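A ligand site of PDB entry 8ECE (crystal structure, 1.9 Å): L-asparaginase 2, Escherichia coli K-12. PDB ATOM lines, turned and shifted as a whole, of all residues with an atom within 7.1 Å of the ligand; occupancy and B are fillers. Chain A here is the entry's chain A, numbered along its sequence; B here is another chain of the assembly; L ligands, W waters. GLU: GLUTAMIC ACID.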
ATOM      1  N   GLY A  18      12.873  20.266  11.883  1.00  0.00           N
ATOM      2  CA  GLY A  18      13.319  18.937  12.346  1.00  0.00           C
ATOM      3  C   GLY A  18      14.423  18.283  11.468  1.00  0.00           C
ATOM      4  O   GLY A  18      15.119  19.025  10.670  1.00  0.00           O
ATOM      5  N   GLY A  19      14.646  16.964  11.571  1.00  0.00           N
ATOM      6  CA  GLY A  19      15.892  16.335  11.024  1.00  0.00           C
ATOM      7  C   GLY A  19      17.076  16.456  11.988  1.00  0.00           C
ATOM      8  O   GLY A  19      16.896  16.986  13.103  1.00  0.00           O
ATOM      9  N   THR A  20      18.293  16.039  11.643  1.00  0.00           N
ATOM     10  CA  THR A  20      19.485  15.947  12.582  1.00  0.00           C
ATOM     11  C   THR A  20      20.064  17.350  12.957  1.00  0.00           C
ATOM     12  O   THR A  20      20.596  17.542  14.084  1.00  0.00           O
ATOM     13  CB  THR A  20      20.527  14.939  12.040  1.00  0.00           C
ATOM     14  OG1 THR A  20      20.684  14.996  10.631  1.00  0.00           O
ATOM     15  CG2 THR A  20      20.107  13.507  12.299  1.00  0.00           C
ATOM     16  N   ILE A  21      19.797  18.374  12.174  1.00  0.00           N
ATOM     17  CA  ILE A  21      20.521  19.684  12.220  1.00  0.00           C
ATOM     18  C   ILE A  21      19.778  20.746  13.077  1.00  0.00           C
ATOM     19  O   ILE A  21      19.577  20.578  14.333  1.00  0.00           O
ATOM     20  CB  ILE A  21      20.608  20.022  10.720  1.00  0.00           C
ATOM     21  CG1 ILE A  21      21.834  20.770  10.265  1.00  0.00           C
ATOM     22  CG2 ILE A  21      19.345  20.739  10.275  1.00  0.00           C
ATOM     23  CD1 ILE A  21      21.729  21.114   8.760  1.00  0.00           C
ATOM     24  N   ILE A  64       9.764  17.645  13.290  1.00  0.00           N
ATOM     25  CA  ILE A  64       9.403  16.238  12.953  1.00  0.00           C
ATOM     26  C   ILE A  64      10.512  15.598  12.107  1.00  0.00           C
ATOM     27  O   ILE A  64      11.210  16.352  11.429  1.00  0.00           O
ATOM     28  CB  ILE A  64       8.086  16.169  12.199  1.00  0.00           C
ATOM     29  CG1 ILE A  64       8.065  17.101  10.996  1.00  0.00           C
ATOM     30  CG2 ILE A  64       6.927  16.472  13.161  1.00  0.00           C
ATOM     31  CD1 ILE A  64       6.830  16.880  10.106  1.00  0.00           C
ATOM     32  N   GLY A  65      10.586  14.268  12.171  1.00  0.00           N
ATOM     33  CA  GLY A  65      11.370  13.502  11.189  1.00  0.00           C
ATOM     34  C   GLY A  65      10.732  13.710   9.835  1.00  0.00           C
ATOM     35  O   GLY A  65       9.460  13.734   9.744  1.00  0.00           O
ATOM     36  N   SER A  66      11.507  13.945   8.788  1.00  0.00           N
ATOM     37  CA  SER A  66      10.896  14.296   7.475  1.00  0.00           C
ATOM     38  C   SER A  66      10.147  13.083   6.850  1.00  0.00           C
ATOM     39  O   SER A  66       9.357  13.367   5.914  1.00  0.00           O
ATOM     40  CB  SER A  66      11.828  14.891   6.495  1.00  0.00           C
ATOM     41  OG  SER A  66      12.655  13.898   5.848  1.00  0.00           O
ATOM     42  N   GLN A  67      10.308  11.875   7.359  1.00  0.00           N
ATOM     43  CA  GLN A  67       9.502  10.751   6.946  1.00  0.00           C
ATOM     44  C   GLN A  67       8.015  11.050   7.265  1.00  0.00           C
ATOM     45  O   GLN A  67       7.151  10.350   6.729  1.00  0.00           O
ATOM     46  CB  GLN A  67       9.906   9.412   7.559  1.00  0.00           C
ATOM     47  CG  GLN A  67       9.747   9.233   9.077  1.00  0.00           C
ATOM     48  CD  GLN A  67      10.974   9.683   9.812  1.00  0.00           C
ATOM     49  OE1 GLN A  67      11.643  10.669   9.486  1.00  0.00           O
ATOM     50  NE2 GLN A  67      11.340   8.911  10.812  1.00  0.00           N
ATOM     51  N   ASP A  68       7.779  11.915   8.262  1.00  0.00           N
ATOM     52  CA  ASP A  68       6.395  12.323   8.626  1.00  0.00           C
ATOM     53  C   ASP A  68       5.926  13.634   8.079  1.00  0.00           C
ATOM     54  O   ASP A  68       4.863  14.233   8.479  1.00  0.00           O
ATOM     55  CB  ASP A  68       6.254  12.325  10.141  1.00  0.00           C
ATOM     56  CG  ASP A  68       6.412  10.980  10.750  1.00  0.00           C
ATOM     57  OD1 ASP A  68       6.076  10.008  10.091  1.00  0.00           O
ATOM     58  OD2 ASP A  68       6.725  10.899  11.965  1.00  0.00           O
ATOM     59  N   HIS A  95      15.837  20.739   7.568  1.00  0.00           N
ATOM     60  CA  HIS A  95      14.815  19.692   7.282  1.00  0.00           C
ATOM     61  C   HIS A  95      15.470  18.311   7.260  1.00  0.00           C
ATOM     62  O   HIS A  95      16.661  18.216   6.911  1.00  0.00           O
ATOM     63  CB  HIS A  95      14.232  20.181   5.933  1.00  0.00           C
ATOM     64  CG  HIS A  95      12.992  19.468   5.439  1.00  0.00           C
ATOM     65  ND1 HIS A  95      13.019  18.135   4.989  1.00  0.00           N
ATOM     66  CD2 HIS A  95      11.765  19.941   5.164  1.00  0.00           C
ATOM     67  CE1 HIS A  95      11.782  17.841   4.530  1.00  0.00           C
ATOM     68  NE2 HIS A  95      11.008  18.914   4.645  1.00  0.00           N
ATOM     69  N   GLY A  96      14.676  17.255   7.579  1.00  0.00           N
ATOM     70  CA  GLY A  96      15.199  15.899   7.408  1.00  0.00           C
ATOM     71  C   GLY A  96      15.461  15.618   5.929  1.00  0.00           C
ATOM     72  O   GLY A  96      14.830  16.259   4.985  1.00  0.00           O
ATOM     73  N   THR A  97      16.440  14.769   5.673  1.00  0.00           N
ATOM     74  CA  THR A  97      16.839  14.498   4.273  1.00  0.00           C
ATOM     75  C   THR A  97      15.839  13.621   3.546  1.00  0.00           C
ATOM     76  O   THR A  97      15.788  13.710   2.319  1.00  0.00           O
ATOM     77  CB  THR A  97      18.239  13.873   4.241  1.00  0.00           C
ATOM     78  OG1 THR A  97      18.204  12.658   4.965  1.00  0.00           O
ATOM     79  CG2 THR A  97      19.232  14.851   4.814  1.00  0.00           C
ATOM     80  N   ASP A  98      15.093  12.780   4.264  1.00  0.00           N
ATOM     81  CA  ASP A  98      14.280  11.752   3.590  1.00  0.00           C
ATOM     82  C   ASP A  98      13.251  12.325   2.632  1.00  0.00           C
ATOM     83  O   ASP A  98      13.086  11.741   1.534  1.00  0.00           O
ATOM     84  CB  ASP A  98      13.586  10.822   4.566  1.00  0.00           C
ATOM     85  CG  ASP A  98      14.512   9.927   5.374  1.00  0.00           C
ATOM     86  OD1 ASP A  98      15.732   9.936   5.085  1.00  0.00           O
ATOM     87  OD2 ASP A  98      13.958   9.299   6.311  1.00  0.00           O
ATOM     88  N   THR A  99      12.569  13.479   2.948  1.00  0.00           N
ATOM     89  CA  THR A  99      11.586  14.074   1.994  1.00  0.00           C
ATOM     90  C   THR A  99      11.939  15.532   1.636  1.00  0.00           C
ATOM     91  O   THR A  99      11.118  16.314   1.146  1.00  0.00           O
ATOM     92  CB  THR A  99      10.173  14.014   2.563  1.00  0.00           C
ATOM     93  OG1 THR A  99      10.093  14.761   3.803  1.00  0.00           O
ATOM     94  CG2 THR A  99       9.742  12.608   2.813  1.00  0.00           C
ATOM     95  N   MET A 100      13.179  15.936   1.889  1.00  0.00           N
ATOM     96  CA  MET A 100      13.638  17.275   1.520  1.00  0.00           C
ATOM     97  C   MET A 100      13.349  17.585   0.053  1.00  0.00           C
ATOM     98  O   MET A 100      13.001  18.700  -0.264  1.00  0.00           O
ATOM     99  CB  MET A 100      15.122  17.465   1.839  1.00  0.00           C
ATOM    100  CG  MET A 100      15.547  18.869   1.499  1.00  0.00           C
ATOM    101  SD  MET A 100      16.986  19.411   2.416  1.00  0.00           S
ATOM    102  CE  MET A 100      18.222  18.170   2.009  1.00  0.00           C
ATOM    103  N   GLY A 121      19.987  19.883   5.164  1.00  0.00           N
ATOM    104  CA  GLY A 121      19.895  18.771   6.109  1.00  0.00           C
ATOM    105  C   GLY A 121      21.302  18.171   6.385  1.00  0.00           C
ATOM    106  O   GLY A 121      22.323  18.757   5.961  1.00  0.00           O
ATOM    107  N   ALA A 122      21.326  17.037   7.041  1.00  0.00           N
ATOM    108  CA  ALA A 122      22.561  16.302   7.346  1.00  0.00           C
ATOM    109  C   ALA A 122      22.271  14.805   7.242  1.00  0.00           C
ATOM    110  O   ALA A 122      21.239  14.315   7.753  1.00  0.00           O
ATOM    111  CB  ALA A 122      23.035  16.659   8.736  1.00  0.00           C
ATOM    112  N   MET A 123      23.248  14.087   6.685  1.00  0.00           N
ATOM    113  CA  MET A 123      23.172  12.637   6.576  1.00  0.00           C
ATOM    114  C   MET A 123      23.790  11.936   7.779  1.00  0.00           C
ATOM    115  O   MET A 123      23.564  10.741   7.912  1.00  0.00           O
ATOM    116  CB  MET A 123      23.833  12.190   5.263  1.00  0.00           C
ATOM    117  CG  MET A 123      23.019  12.651   4.053  1.00  0.00           C
ATOM    118  SD  MET A 123      21.465  11.709   3.941  1.00  0.00           S
ATOM    119  CE  MET A 123      22.024  10.018   3.572  1.00  0.00           C
ATOM    120  N   ARG A 124      24.509  12.616   8.654  1.00  0.00           N
ATOM    121  CA  ARG A 124      25.055  11.991   9.835  1.00  0.00           C
ATOM    122  C   ARG A 124      24.484  12.710  11.059  1.00  0.00           C
ATOM    123  O   ARG A 124      24.332  13.925  11.027  1.00  0.00           O
ATOM    124  CB  ARG A 124      26.602  12.043   9.864  1.00  0.00           C
ATOM    125  CG  ARG A 124      27.246  11.258   8.716  1.00  0.00           C
ATOM    126  CD  ARG A 124      28.730  11.539   8.687  1.00  0.00           C
ATOM    127  NE  ARG A 124      29.362  10.679   7.636  1.00  0.00           N
ATOM    128  CZ  ARG A 124      30.519  10.917   7.103  1.00  0.00           C
ATOM    129  NH1 ARG A 124      31.209  12.018   7.436  1.00  0.00           N
ATOM    130  NH2 ARG A 124      30.970  10.113   6.107  1.00  0.00           N
ATOM    131  N   LYS A 170      17.423  12.472  -3.579  1.00  0.00           N
ATOM    132  CA  LYS A 170      18.283  11.655  -2.702  1.00  0.00           C
ATOM    133  C   LYS A 170      18.620  10.361  -3.448  1.00  0.00           C
ATOM    134  O   LYS A 170      17.734   9.575  -3.724  1.00  0.00           O
ATOM    135  CB  LYS A 170      17.537  11.390  -1.396  1.00  0.00           C
ATOM    136  CG  LYS A 170      18.393  10.616  -0.397  1.00  0.00           C
ATOM    137  CD  LYS A 170      17.721  10.547   1.004  1.00  0.00           C
ATOM    138  CE  LYS A 170      18.617  10.504   2.151  1.00  0.00           C
ATOM    139  NZ  LYS A 170      17.894  10.470   3.426  1.00  0.00           N
ATOM    140  N   VAL B 252      11.261   5.942   2.522  1.00  0.00           N
ATOM    141  CA  VAL B 252      12.041   7.140   2.259  1.00  0.00           C
ATOM    142  C   VAL B 252      13.405   6.987   2.920  1.00  0.00           C
ATOM    143  O   VAL B 252      13.490   6.411   4.007  1.00  0.00           O
ATOM    144  CB  VAL B 252      11.271   8.417   2.670  1.00  0.00           C
ATOM    145  CG1 VAL B 252       9.969   8.572   1.848  1.00  0.00           C
ATOM    146  CG2 VAL B 252      10.973   8.472   4.174  1.00  0.00           C
ATOM    147  N   GLY B 253      14.426   7.567   2.321  1.00  0.00           N
ATOM    148  CA  GLY B 253      15.783   7.481   2.889  1.00  0.00           C
ATOM    149  C   GLY B 253      16.149   6.039   3.207  1.00  0.00           C
ATOM    150  O   GLY B 253      15.939   5.084   2.346  1.00  0.00           O
ATOM    151  N   ASN B 254      16.603   5.813   4.421  1.00  0.00           N
ATOM    152  CA  ASN B 254      17.058   4.503   4.862  1.00  0.00           C
ATOM    153  C   ASN B 254      15.883   3.595   5.290  1.00  0.00           C
ATOM    154  O   ASN B 254      15.792   3.195   6.503  1.00  0.00           O
ATOM    155  CB  ASN B 254      18.179   4.664   5.880  1.00  0.00           C
ATOM    156  CG  ASN B 254      18.942   3.399   6.136  1.00  0.00           C
ATOM    157  OD1 ASN B 254      18.558   2.298   5.777  1.00  0.00           O
ATOM    158  ND2 ASN B 254      20.004   3.534   6.936  1.00  0.00           N
ATOM    159  N   ASN B 256      12.707   4.360   5.745  1.00  0.00           N
ATOM    160  CA  ASN B 256      11.792   4.940   6.760  1.00  0.00           C
ATOM    161  C   ASN B 256      10.359   4.956   6.217  1.00  0.00           C
ATOM    162  O   ASN B 256      10.139   4.989   4.950  1.00  0.00           O
ATOM    163  CB  ASN B 256      12.256   6.324   7.189  1.00  0.00           C
ATOM    164  CG  ASN B 256      13.591   6.206   7.919  1.00  0.00           C
ATOM    165  OD1 ASN B 256      14.628   6.844   7.614  1.00  0.00           O
ATOM    166  ND2 ASN B 256      13.541   5.364   8.888  1.00  0.00           N
ATOM    167  N   GLU B 291      17.333   3.865  12.009  1.00  0.00           N
ATOM    168  CA  GLU B 291      16.285   4.422  12.808  1.00  0.00           C
ATOM    169  C   GLU B 291      15.228   3.482  13.225  1.00  0.00           C
ATOM    170  O   GLU B 291      14.504   3.719  14.175  1.00  0.00           O
ATOM    171  CB  GLU B 291      15.621   5.593  12.149  1.00  0.00           C
ATOM    172  CG  GLU B 291      16.370   6.874  12.243  1.00  0.00           C
ATOM    173  CD  GLU B 291      15.559   7.965  11.514  1.00  0.00           C
ATOM    174  OE1 GLU B 291      14.655   8.534  12.140  1.00  0.00           O
ATOM    175  OE2 GLU B 291      15.791   8.169  10.320  1.00  0.00           O
HETATM  176  N   GLU L   1      14.310  10.127   8.963  1.00  0.00           N
HETATM  177  CA  GLU L   1      15.120  11.284   9.271  1.00  0.00           C
HETATM  178  C   GLU L   1      14.567  12.505   8.584  1.00  0.00           C
HETATM  179  O   GLU L   1      14.475  12.579   7.365  1.00  0.00           O
HETATM  180  CB  GLU L   1      16.574  11.059   8.849  1.00  0.00           C
HETATM  181  CG  GLU L   1      17.564  11.962   9.566  1.00  0.00           C
HETATM  182  CD  GLU L   1      17.750  13.291   8.874  1.00  0.00           C
HETATM  183  OE1 GLU L   1      17.873  13.314   7.634  1.00  0.00           O
HETATM  184  OE2 GLU L   1      17.775  14.318   9.556  1.00  0.00           O
HETATM  185  OXT GLU L   1      14.201  13.447   9.259  1.00  0.00           O
HETATM  186  O   HOH W   1      17.086  12.809  12.799  1.00  0.00           O
HETATM  187  O   HOH W   2      19.928  11.626   7.468  1.00  0.00           O
HETATM  188  O   HOH W   3      18.667  16.720   8.198  1.00  0.00           O
HETATM  189  O   HOH W   4      14.650  13.231  12.032  1.00  0.00           O
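The backbone NH (N) of Ser 66 sits at hydrogen-bond distance from an oxygen (OXT) of the ligand.
O of the ligand is in hydrogen-bond range of OG of Ser 66 (2.7 Å).
An oxygen (OE2) of the ligand sits at hydrogen-bond distance from the backbone NH (N) of Thr 20, at 2.8 Å.
An oxygen (OE2) of the ligand sits at hydrogen-bond distance from the side-chain hydroxyl (OG1) of Thr 20 (3.2 Å).
N of Thr 97 is in hydrogen-bond range of OE1 of the ligand (2.8 Å).
An oxygen (OE1) of the ligand sits at hydrogen-bond distance from the side-chain hydroxyl (OG1) of Thr 97 (2.8 Å).
A nitrogen (N) of the ligand sits at hydrogen-bond distance from the side-chain amide oxygen of Gln 67 (2.8 Å).
N of Asp 98 lies within hydrogen-bond range of O of the ligand (3.2 Å).
OD2 of Asp 98 is in salt-bridge range of N of the ligand.
OE2 of Glu 291 of chain B is in salt-bridge range of N of the ligand.
The side-chain hydroxyl (OG) of Ser 66 sits at hydrogen-bond distance from the backbone NH (N) of Asp 98 (3.1 Å).
The backbone carbonyl oxygen (O) of Gly 96 lies close to the side-chain hydroxyl (OG) of Ser 66, at 3.3 Å.
OG1 of Thr 99 is in hydrogen-bond range of O of Ser 66.
The side-chain hydroxyl (OG1) of Thr 20 lies within hydrogen-bond range of the backbone carbonyl oxygen (O) of Ala 122, 3.0 Å away.
The side-chain carboxylate (OD2) of Asp 98 lies close to the side-chain amide oxygen (OD1) of Asn 256 of chain B, 2.9 Å away.
The side-chain amino group (NZ) of Lys 170 is in salt-bridge range of the side-chain carboxylate (OD1) of Asp 98.
OE2 of Glu 291 of chain B sits close to OD1 of Asn 256 of chain B, at 3.2 Å.
N of Gly 19 is in hydrogen-bond range of O of Ile 64 (3.5 Å).
Gly 19 touches the ligand.
Gly 65 touches the ligand (CA to OXT, 3.4 Å).
Gly 96 touches the ligand (CA to OXT, 3.2 Å).
Ala 122 touches the ligand (O to OE1, 3.5 Å).
OD1 of Asn 256 of chain B touches N of the ligand (3.6 Å).
Within 4 Å of the ligand: Gly 19, Thr 20, Gly 65, Ser 66, Gln 67, Gly 96, Thr 97, Asp 98, Ala 122, Asn 256 of chain B and Glu 291 of chain B.
Water W2 lies within hydrogen-bond range of an oxygen (OE1) of the ligand, the backbone carbonyl oxygen of Ala 122 and the side-chain hydroxyl of Thr 97.
Water W3 lies within hydrogen-bond range of O of His 95, OE2 of the ligand and N of Ala 122.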
